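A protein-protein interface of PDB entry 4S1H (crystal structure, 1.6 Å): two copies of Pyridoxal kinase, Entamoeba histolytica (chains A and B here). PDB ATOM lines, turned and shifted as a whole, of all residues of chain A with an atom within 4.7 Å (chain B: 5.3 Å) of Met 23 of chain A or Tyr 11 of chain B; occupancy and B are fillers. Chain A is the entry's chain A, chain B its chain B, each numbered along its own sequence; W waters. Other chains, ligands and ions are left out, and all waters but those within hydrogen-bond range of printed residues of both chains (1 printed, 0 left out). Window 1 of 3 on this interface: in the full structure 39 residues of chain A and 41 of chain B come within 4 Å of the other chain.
The side-chain hydroxyl (OG1) of Thr 39 of chain B lies within hydrogen-bond range of the backbone NH (N) of Tyr 11 of chain B (2.9 Å).
The backbone carbonyl oxygen (O) of Tyr 11 of chain B is in hydrogen-bond range of the backbone NH (N) of Leu 41 of chain B (3.1 Å).
NE2 of His 40 of chain B sits at hydrogen-bond distance from SG of Cys 13 of chain B, 3.4 Å away.
O of Leu 41 of chain B sits at hydrogen-bond distance from N of Cys 13 of chain B (2.8 Å).
Water W1 bridges OD2 of Asp 27 of chain A (2.7 Å) and OD2 of Asp 27 of chain B (2.7 Å).
Tyr 11 of chain B touches three residues of chain A.
Of the printed residues of chain B, Tyr 11 of chain A touches Leu 37.
Printed residues of chain A within 4 Å of Met 23 of chain B: Arg 20 (3.1 Å) and Met 23 (3.0 Å).
Of the printed residues of chain A, His 40 of chain B touches Leu 37 (3.2 Å).
The nearest residue of chain B that does not touch Met 23 of chain A is Asp 27 of chain B (5.2 Å).
The nearest printed residue of chain A that does not touch Tyr 11 of chain B is Tyr 11 of chain A (5.2 Å).
Among the printed residues, pairs that only touch across the chains: Arg 20 of chain A with Met 23 of chain B, Met 23 of chain A with Tyr 11 of chain B, Phe 35 of chain A with Arg 20 of chain B, Ile 24 of chain A with Asp 27 of chain B, Leu 37 of chain A with Leu 37 of chain B, Tyr 11 of chain A with Leu 37 of chain B, Leu 37 of chain A with Tyr 11 of chain B and Met 23 of chain A with Arg 20 of chain B.
Of the 13 printed residues of chain A, 7 touch a printed residue of chain B.
Along chain A the printed residues that touch a printed residue of chain B span positions 11 to 37.
Of the 14 printed residues of chain B, 7 touch a printed residue of chain A.
Among the printed residues, Asp or Glu carboxylates within 4 Å of a Lys or Arg side-chain nitrogen of the other chain: Arg 20 of chain A with Asp 27 of chain B (2.9 Å) and Asp 27 of chain A with Arg 20 of chain B (2.9 Å).
The guanidinium group (NH2) of Arg 20 of chain A is in salt-bridge range of the side-chain carboxylate (OD1) of Asp 27 of chain B (2.9 Å).
The side-chain carboxylate of Asp 27 of chain A is in salt-bridge range of the guanidinium group of Arg 20 of chain B (2.9 Å).
OH of Tyr 11 of chain B sits at hydrogen-bond distance from O of Phe 35 of chain A (2.7 Å).
The backbone NH (N) of Phe 35 of chain A lies within hydrogen-bond range of the backbone carbonyl oxygen (O) of Cys 13 of chain B (2.9 Å).
NE2 of His 40 of chain B sits at hydrogen-bond distance from N of Leu 37 of chain A, at 3.2 Å.
The side-chain sulfur of Met 23 of chain B lies close to the side-chain sulfur of Met 23 of chain A (3.7 Å).
Tyr 11 of chain A touches Leu 37 of chain B, and with the chains exchanged Leu 37 of chain A touches Tyr 11 of chain B.
Arg 20 of chain A touches Met 23 of chain B, and with the chains exchanged Met 23 of chain A touches Arg 20 of chain B.
Arg 20 of chain A touches Asp 27 of chain B, and with the chains exchanged Asp 27 of chain A touches Arg 20 of chain B.
Leu 37 of chain B touches its own counterpart, Leu 37 of chain A.
Positions printed for both chains: 11, 19, 20, 23, 27 and 37.
Of the 14 pairs that touch across the chains among the printed residues, 8 have their exchanged pair printed and touching as well.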
ATOM      1  N   TYR A  11      -3.066  25.044 -16.655  1.00  0.00           N
ATOM      2  CA  TYR A  11      -3.229  25.439 -15.263  1.00  0.00           C
ATOM      3  C   TYR A  11      -1.937  25.185 -14.492  1.00  0.00           C
ATOM      4  O   TYR A  11      -1.329  24.117 -14.650  1.00  0.00           O
ATOM      5  CB  TYR A  11      -4.405  24.686 -14.621  1.00  0.00           C
ATOM      6  CG  TYR A  11      -4.586  25.047 -13.182  1.00  0.00           C
ATOM      7  CD1 TYR A  11      -5.339  26.131 -12.829  1.00  0.00           C
ATOM      8  CD2 TYR A  11      -3.953  24.320 -12.176  1.00  0.00           C
ATOM      9  CE1 TYR A  11      -5.478  26.522 -11.517  1.00  0.00           C
ATOM     10  CE2 TYR A  11      -4.097  24.676 -10.838  1.00  0.00           C
ATOM     11  CZ  TYR A  11      -4.888  25.760 -10.522  1.00  0.00           C
ATOM     12  OH  TYR A  11      -5.050  26.176  -9.222  1.00  0.00           O
ATOM     13  N   ASN A  19      -4.860  29.413 -18.205  1.00  0.00           N
ATOM     14  CA  ASN A  19      -6.166  29.626 -17.575  1.00  0.00           C
ATOM     15  C   ASN A  19      -6.130  30.255 -16.176  1.00  0.00           C
ATOM     16  O   ASN A  19      -7.120  30.832 -15.763  1.00  0.00           O
ATOM     17  CB  ASN A  19      -7.023  28.349 -17.558  1.00  0.00           C
ATOM     18  CG  ASN A  19      -8.086  28.338 -18.623  1.00  0.00           C
ATOM     19  OD1 ASN A  19      -8.383  29.359 -19.242  1.00  0.00           O
ATOM     20  ND2 ASN A  19      -8.679  27.191 -18.836  1.00  0.00           N
ATOM     21  N   ARG A  20      -5.011  30.186 -15.472  1.00  0.00           N
ATOM     22  CA  ARG A  20      -4.869  30.902 -14.214  1.00  0.00           C
ATOM     23  C   ARG A  20      -4.889  32.423 -14.428  1.00  0.00           C
ATOM     24  O   ARG A  20      -5.578  33.144 -13.707  1.00  0.00           O
ATOM     25  CB  ARG A  20      -3.656  30.415 -13.450  1.00  0.00           C
ATOM     26  CG  ARG A  20      -3.520  30.916 -12.059  1.00  0.00           C
ATOM     27  CD  ARG A  20      -4.482  30.290 -11.038  1.00  0.00           C
ATOM     28  NE  ARG A  20      -4.278  31.139  -9.856  1.00  0.00           N
ATOM     29  CZ  ARG A  20      -5.118  32.033  -9.332  1.00  0.00           C
ATOM     30  NH1 ARG A  20      -6.363  32.199  -9.793  1.00  0.00           N
ATOM     31  NH2 ARG A  20      -4.683  32.792  -8.345  1.00  0.00           N
ATOM     32  N   CYS A  21      -4.138  32.914 -15.420  1.00  0.00           N
ATOM     33  CA  CYS A  21      -4.287  34.311 -15.896  1.00  0.00           C
ATOM     34  C   CYS A  21      -5.720  34.620 -16.286  1.00  0.00           C
ATOM     35  O   CYS A  21      -6.251  35.666 -15.939  1.00  0.00           O
ATOM     36  CB  CYS A  21      -3.372  34.596 -17.085  1.00  0.00           C
ATOM     37  SG  CYS A  21      -1.648  34.506 -16.641  1.00  0.00           S
ATOM     38  N   GLY A  22      -6.346  33.704 -17.021  1.00  0.00           N
ATOM     39  CA  GLY A  22      -7.701  33.875 -17.474  1.00  0.00           C
ATOM     40  C   GLY A  22      -8.664  34.018 -16.324  1.00  0.00           C
ATOM     41  O   GLY A  22      -9.520  34.896 -16.342  1.00  0.00           O
ATOM     42  N   MET A  23      -8.476  33.216 -15.299  1.00  0.00           N
ATOM     43  CA  MET A  23      -9.390  33.291 -14.148  1.00  0.00           C
ATOM     44  C   MET A  23      -9.274  34.650 -13.474  1.00  0.00           C
ATOM     45  O   MET A  23     -10.267  35.303 -13.174  1.00  0.00           O
ATOM     46  CB  MET A  23      -9.093  32.167 -13.149  1.00  0.00           C
ATOM     47  CG  MET A  23      -9.326  30.750 -13.686  1.00  0.00           C
ATOM     48  SD  MET A  23      -8.606  29.395 -12.665  1.00  0.00           S
ATOM     49  CE  MET A  23      -8.782  28.018 -13.772  1.00  0.00           C
ATOM     50  N   ILE A  24      -8.043  35.069 -13.192  1.00  0.00           N
ATOM     51  CA  ILE A  24      -7.796  36.309 -12.501  1.00  0.00           C
ATOM     52  C   ILE A  24      -8.409  37.472 -13.286  1.00  0.00           C
ATOM     53  O   ILE A  24      -9.070  38.340 -12.715  1.00  0.00           O
ATOM     54  CB  ILE A  24      -6.286  36.550 -12.295  1.00  0.00           C
ATOM     55  CG1 ILE A  24      -5.734  35.524 -11.306  1.00  0.00           C
ATOM     56  CG2 ILE A  24      -6.015  37.972 -11.791  1.00  0.00           C
ATOM     57  CD1 ILE A  24      -4.222  35.387 -11.369  1.00  0.00           C
ATOM     58  N   ILE A  25      -8.170  37.489 -14.596  1.00  0.00           N
ATOM     59  CA  ILE A  25      -8.578  38.626 -15.416  1.00  0.00           C
ATOM     60  C   ILE A  25     -10.106  38.637 -15.624  1.00  0.00           C
ATOM     61  O   ILE A  25     -10.765  39.649 -15.372  1.00  0.00           O
ATOM     62  CB  ILE A  25      -7.796  38.690 -16.742  1.00  0.00           C
ATOM     63  CG1 ILE A  25      -6.322  38.867 -16.403  1.00  0.00           C
ATOM     64  CG2 ILE A  25      -8.339  39.817 -17.605  1.00  0.00           C
ATOM     65  CD1 ILE A  25      -5.359  38.506 -17.522  1.00  0.00           C
ATOM     66  N   LEU A  26     -10.650  37.534 -16.106  1.00  0.00           N
ATOM     67  CA  LEU A  26     -12.105  37.438 -16.351  1.00  0.00           C
ATOM     68  C   LEU A  26     -12.900  37.579 -15.054  1.00  0.00           C
ATOM     69  O   LEU A  26     -13.935  38.266 -15.042  1.00  0.00           O
ATOM     70  CB  LEU A  26     -12.458  36.152 -17.087  1.00  0.00           C
ATOM     71  CG  LEU A  26     -11.991  36.077 -18.540  1.00  0.00           C
ATOM     72  CD1 LEU A  26     -12.044  34.667 -19.104  1.00  0.00           C
ATOM     73  CD2 LEU A  26     -12.773  37.026 -19.440  1.00  0.00           C
ATOM     74  N   ASP A  27     -12.412  37.004 -13.966  1.00  0.00           N
ATOM     75  CA  ASP A  27     -13.066  37.250 -12.649  1.00  0.00           C
ATOM     76  C   ASP A  27     -13.073  38.767 -12.303  1.00  0.00           C
ATOM     77  O   ASP A  27     -14.104  39.318 -11.888  1.00  0.00           O
ATOM     78  CB  ASP A  27     -12.425  36.450 -11.472  1.00  0.00           C
ATOM     79  CG  ASP A  27     -12.581  34.895 -11.589  1.00  0.00           C
ATOM     80  OD1 ASP A  27     -13.349  34.368 -12.437  1.00  0.00           O
ATOM     81  OD2 ASP A  27     -11.881  34.169 -10.813  1.00  0.00           O
ATOM     82  N   SER A  28     -11.953  39.464 -12.502  1.00  0.00           N
ATOM     83  CA  SER A  28     -11.871  40.878 -12.164  1.00  0.00           C
ATOM     84  C   SER A  28     -12.781  41.760 -13.045  1.00  0.00           C
ATOM     85  O   SER A  28     -13.247  42.794 -12.611  1.00  0.00           O
ATOM     86  CB  SER A  28     -10.418  41.393 -12.193  1.00  0.00           C
ATOM     87  OG  SER A  28     -10.251  42.420 -13.155  1.00  0.00           O
ATOM     88  N   PHE A  35     -13.749  27.467 -17.181  1.00  0.00           N
ATOM     89  CA  PHE A  35     -12.308  27.265 -17.313  1.00  0.00           C
ATOM     90  C   PHE A  35     -11.982  25.774 -17.337  1.00  0.00           C
ATOM     91  O   PHE A  35     -11.878  25.116 -16.273  1.00  0.00           O
ATOM     92  CB  PHE A  35     -11.525  27.976 -16.208  1.00  0.00           C
ATOM     93  CG  PHE A  35     -11.790  29.445 -16.118  1.00  0.00           C
ATOM     94  CD1 PHE A  35     -12.856  29.947 -15.354  1.00  0.00           C
ATOM     95  CD2 PHE A  35     -10.990  30.355 -16.812  1.00  0.00           C
ATOM     96  CE1 PHE A  35     -13.093  31.319 -15.279  1.00  0.00           C
ATOM     97  CE2 PHE A  35     -11.225  31.720 -16.694  1.00  0.00           C
ATOM     98  CZ  PHE A  35     -12.289  32.200 -15.972  1.00  0.00           C
ATOM     99  N   LEU A  37      -9.407  22.962 -17.959  1.00  0.00           N
ATOM    100  CA  LEU A  37      -7.934  22.851 -17.894  1.00  0.00           C
ATOM    101  C   LEU A  37      -7.364  21.810 -18.856  1.00  0.00           C
ATOM    102  O   LEU A  37      -7.944  20.763 -19.105  1.00  0.00           O
ATOM    103  CB  LEU A  37      -7.493  22.519 -16.457  1.00  0.00           C
ATOM    104  CG  LEU A  37      -8.165  23.364 -15.364  1.00  0.00           C
ATOM    105  CD1 LEU A  37      -7.560  22.961 -14.020  1.00  0.00           C
ATOM    106  CD2 LEU A  37      -8.080  24.864 -15.609  1.00  0.00           C
ATOM    107  N   SER B   9      -7.915  21.599  -2.436  1.00  0.00           N
ATOM    108  CA  SER B   9      -9.351  21.374  -2.497  1.00  0.00           C
ATOM    109  C   SER B   9      -9.788  21.139  -3.947  1.00  0.00           C
ATOM    110  O   SER B   9      -8.972  21.108  -4.871  1.00  0.00           O
ATOM    111  CB  SER B   9     -10.137  22.521  -1.881  1.00  0.00           C
ATOM    112  OG  SER B   9     -11.514  22.183  -1.715  1.00  0.00           O
ATOM    113  N   SER B  10     -11.098  21.019  -4.145  1.00  0.00           N
ATOM    114  CA  SER B  10     -11.639  20.572  -5.415  1.00  0.00           C
ATOM    115  C   SER B  10     -11.620  21.703  -6.439  1.00  0.00           C
ATOM    116  O   SER B  10     -11.495  22.862  -6.094  1.00  0.00           O
ATOM    117  CB  SER B  10     -13.089  20.131  -5.248  1.00  0.00           C
ATOM    118  OG  SER B  10     -13.805  21.136  -4.541  1.00  0.00           O
ATOM    119  N   TYR B  11     -11.765  21.319  -7.706  1.00  0.00           N
ATOM    120  CA  TYR B  11     -11.880  22.259  -8.779  1.00  0.00           C
ATOM    121  C   TYR B  11     -13.036  21.864  -9.689  1.00  0.00           C
ATOM    122  O   TYR B  11     -13.200  20.688 -10.025  1.00  0.00           O
ATOM    123  CB  TYR B  11     -10.582  22.333  -9.602  1.00  0.00           C
ATOM    124  CG  TYR B  11     -10.674  23.271 -10.775  1.00  0.00           C
ATOM    125  CD1 TYR B  11     -10.443  24.592 -10.577  1.00  0.00           C
ATOM    126  CD2 TYR B  11     -11.083  22.816 -11.999  1.00  0.00           C
ATOM    127  CE1 TYR B  11     -10.566  25.492 -11.616  1.00  0.00           C
ATOM    128  CE2 TYR B  11     -11.251  23.690 -13.057  1.00  0.00           C
ATOM    129  CZ  TYR B  11     -10.967  25.019 -12.845  1.00  0.00           C
ATOM    130  OH  TYR B  11     -11.088  25.939 -13.858  1.00  0.00           O
ATOM    131  N   VAL B  12     -13.826  22.871 -10.082  1.00  0.00           N
ATOM    132  CA  VAL B  12     -14.897  22.727 -11.060  1.00  0.00           C
ATOM    133  C   VAL B  12     -14.674  23.734 -12.170  1.00  0.00           C
ATOM    134  O   VAL B  12     -14.342  24.872 -11.863  1.00  0.00           O
ATOM    135  CB  VAL B  12     -16.326  22.931 -10.453  1.00  0.00           C
ATOM    136  CG1 VAL B  12     -16.663  21.731  -9.590  1.00  0.00           C
ATOM    137  CG2 VAL B  12     -16.483  24.222  -9.633  1.00  0.00           C
ATOM    138  N   CYS B  13     -14.862  23.310 -13.414  1.00  0.00           N
ATOM    139  CA  CYS B  13     -14.675  24.181 -14.568  1.00  0.00           C
ATOM    140  C   CYS B  13     -15.732  25.251 -14.641  1.00  0.00           C
ATOM    141  O   CYS B  13     -15.468  26.358 -15.124  1.00  0.00           O
ATOM    142  CB  CYS B  13     -14.669  23.356 -15.873  1.00  0.00           C
ATOM    143  SG  CYS B  13     -13.352  22.138 -15.910  1.00  0.00           S
ATOM    144  N   ASN B  19     -11.727  25.041  -4.343  1.00  0.00           N
ATOM    145  CA  ASN B  19     -10.667  25.953  -4.748  1.00  0.00           C
ATOM    146  C   ASN B  19     -11.074  27.020  -5.720  1.00  0.00           C
ATOM    147  O   ASN B  19     -10.395  28.033  -5.794  1.00  0.00           O
ATOM    148  CB  ASN B  19      -9.385  25.211  -5.202  1.00  0.00           C
ATOM    149  CG  ASN B  19      -8.335  25.153  -4.126  1.00  0.00           C
ATOM    150  OD1 ASN B  19      -8.417  25.853  -3.112  1.00  0.00           O
ATOM    151  ND2 ASN B  19      -7.339  24.309  -4.330  1.00  0.00           N
ATOM    152  N   ARG B  20     -12.141  26.818  -6.495  1.00  0.00           N
ATOM    153  CA  ARG B  20     -12.631  27.868  -7.369  1.00  0.00           C
ATOM    154  C   ARG B  20     -13.183  29.054  -6.560  1.00  0.00           C
ATOM    155  O   ARG B  20     -12.868  30.178  -6.828  1.00  0.00           O
ATOM    156  CB  ARG B  20     -13.636  27.276  -8.333  1.00  0.00           C
ATOM    157  CG  ARG B  20     -14.051  28.173  -9.433  1.00  0.00           C
ATOM    158  CD  ARG B  20     -12.978  28.389 -10.508  1.00  0.00           C
ATOM    159  NE  ARG B  20     -13.557  29.462 -11.265  1.00  0.00           N
ATOM    160  CZ  ARG B  20     -13.165  30.735 -11.294  1.00  0.00           C
ATOM    161  NH1 ARG B  20     -12.058  31.167 -10.693  1.00  0.00           N
ATOM    162  NH2 ARG B  20     -13.922  31.588 -11.967  1.00  0.00           N
ATOM    163  N   MET B  23     -10.074  30.729  -5.089  1.00  0.00           N
ATOM    164  CA  MET B  23      -9.351  31.583  -6.018  1.00  0.00           C
ATOM    165  C   MET B  23     -10.037  32.932  -6.095  1.00  0.00           C
ATOM    166  O   MET B  23      -9.391  33.968  -6.036  1.00  0.00           O
ATOM    167  CB  MET B  23      -9.295  30.926  -7.386  1.00  0.00           C
ATOM    168  CG  MET B  23      -8.495  29.598  -7.449  1.00  0.00           C
ATOM    169  SD  MET B  23      -8.679  28.652  -9.022  1.00  0.00           S
ATOM    170  CE  MET B  23      -8.661  30.187  -9.763  1.00  0.00           C
ATOM    171  N   ASP B  27      -7.993  35.889  -4.466  1.00  0.00           N
ATOM    172  CA  ASP B  27      -7.579  36.848  -5.501  1.00  0.00           C
ATOM    173  C   ASP B  27      -8.165  38.243  -5.221  1.00  0.00           C
ATOM    174  O   ASP B  27      -7.468  39.253  -5.263  1.00  0.00           O
ATOM    175  CB  ASP B  27      -7.985  36.401  -6.929  1.00  0.00           C
ATOM    176  CG  ASP B  27      -7.222  35.130  -7.433  1.00  0.00           C
ATOM    177  OD1 ASP B  27      -6.238  34.651  -6.796  1.00  0.00           O
ATOM    178  OD2 ASP B  27      -7.633  34.570  -8.488  1.00  0.00           O
ATOM    179  N   LEU B  37      -5.136  21.427  -6.803  1.00  0.00           N
ATOM    180  CA  LEU B  37      -6.436  20.800  -7.026  1.00  0.00           C
ATOM    181  C   LEU B  37      -6.490  19.325  -6.582  1.00  0.00           C
ATOM    182  O   LEU B  37      -5.545  18.555  -6.766  1.00  0.00           O
ATOM    183  CB  LEU B  37      -6.815  20.924  -8.497  1.00  0.00           C
ATOM    184  CG  LEU B  37      -6.589  22.321  -9.118  1.00  0.00           C
ATOM    185  CD1 LEU B  37      -7.100  22.323 -10.537  1.00  0.00           C
ATOM    186  CD2 LEU B  37      -7.218  23.444  -8.272  1.00  0.00           C
ATOM    187  N   THR B  38      -7.641  18.925  -6.048  1.00  0.00           N
ATOM    188  CA  THR B  38      -7.876  17.503  -5.768  1.00  0.00           C
ATOM    189  C   THR B  38      -8.807  16.834  -6.780  1.00  0.00           C
ATOM    190  O   THR B  38      -8.995  15.597  -6.744  1.00  0.00           O
ATOM    191  CB  THR B  38      -8.492  17.304  -4.387  1.00  0.00           C
ATOM    192  OG1 THR B  38      -9.744  17.988  -4.333  1.00  0.00           O
ATOM    193  CG2 THR B  38      -7.592  17.856  -3.316  1.00  0.00           C
ATOM    194  N   THR B  39      -9.442  17.643  -7.614  1.00  0.00           N
ATOM    195  CA  THR B  39     -10.287  17.157  -8.692  1.00  0.00           C
ATOM    196  C   THR B  39     -10.183  18.078  -9.864  1.00  0.00           C
ATOM    197  O   THR B  39      -9.756  19.227  -9.721  1.00  0.00           O
ATOM    198  CB  THR B  39     -11.780  17.165  -8.331  1.00  0.00           C
ATOM    199  OG1 THR B  39     -12.258  18.514  -8.185  1.00  0.00           O
ATOM    200  CG2 THR B  39     -12.067  16.443  -7.070  1.00  0.00           C
ATOM    201  N   HIS B  40     -10.612  17.568 -11.009  1.00  0.00           N
ATOM    202  CA  HIS B  40     -10.856  18.402 -12.191  1.00  0.00           C
ATOM    203  C   HIS B  40     -12.190  17.957 -12.758  1.00  0.00           C
ATOM    204  O   HIS B  40     -12.254  17.069 -13.608  1.00  0.00           O
ATOM    205  CB  HIS B  40      -9.697  18.275 -13.196  1.00  0.00           C
ATOM    206  CG  HIS B  40      -9.878  19.063 -14.466  1.00  0.00           C
ATOM    207  ND1 HIS B  40      -9.320  18.664 -15.661  1.00  0.00           N
ATOM    208  CD2 HIS B  40     -10.526  20.220 -14.724  1.00  0.00           C
ATOM    209  CE1 HIS B  40      -9.612  19.544 -16.605  1.00  0.00           C
ATOM    210  NE2 HIS B  40     -10.348  20.496 -16.069  1.00  0.00           N
ATOM    211  N   LEU B  41     -13.256  18.592 -12.293  1.00  0.00           N
ATOM    212  CA  LEU B  41     -14.601  18.237 -12.681  1.00  0.00           C
ATOM    213  C   LEU B  41     -15.218  19.313 -13.536  1.00  0.00           C
ATOM    214  O   LEU B  41     -14.906  20.475 -13.362  1.00  0.00           O
ATOM    215  CB  LEU B  41     -15.497  18.046 -11.425  1.00  0.00           C
ATOM    216  CG  LEU B  41     -14.927  17.118 -10.350  1.00  0.00           C
ATOM    217  CD1 LEU B  41     -15.811  17.078  -9.113  1.00  0.00           C
ATOM    218  CD2 LEU B  41     -14.730  15.720 -10.902  1.00  0.00           C
HETATM  219  O   HOH W   1     -10.016  35.452  -9.435  1.00  0.00           O
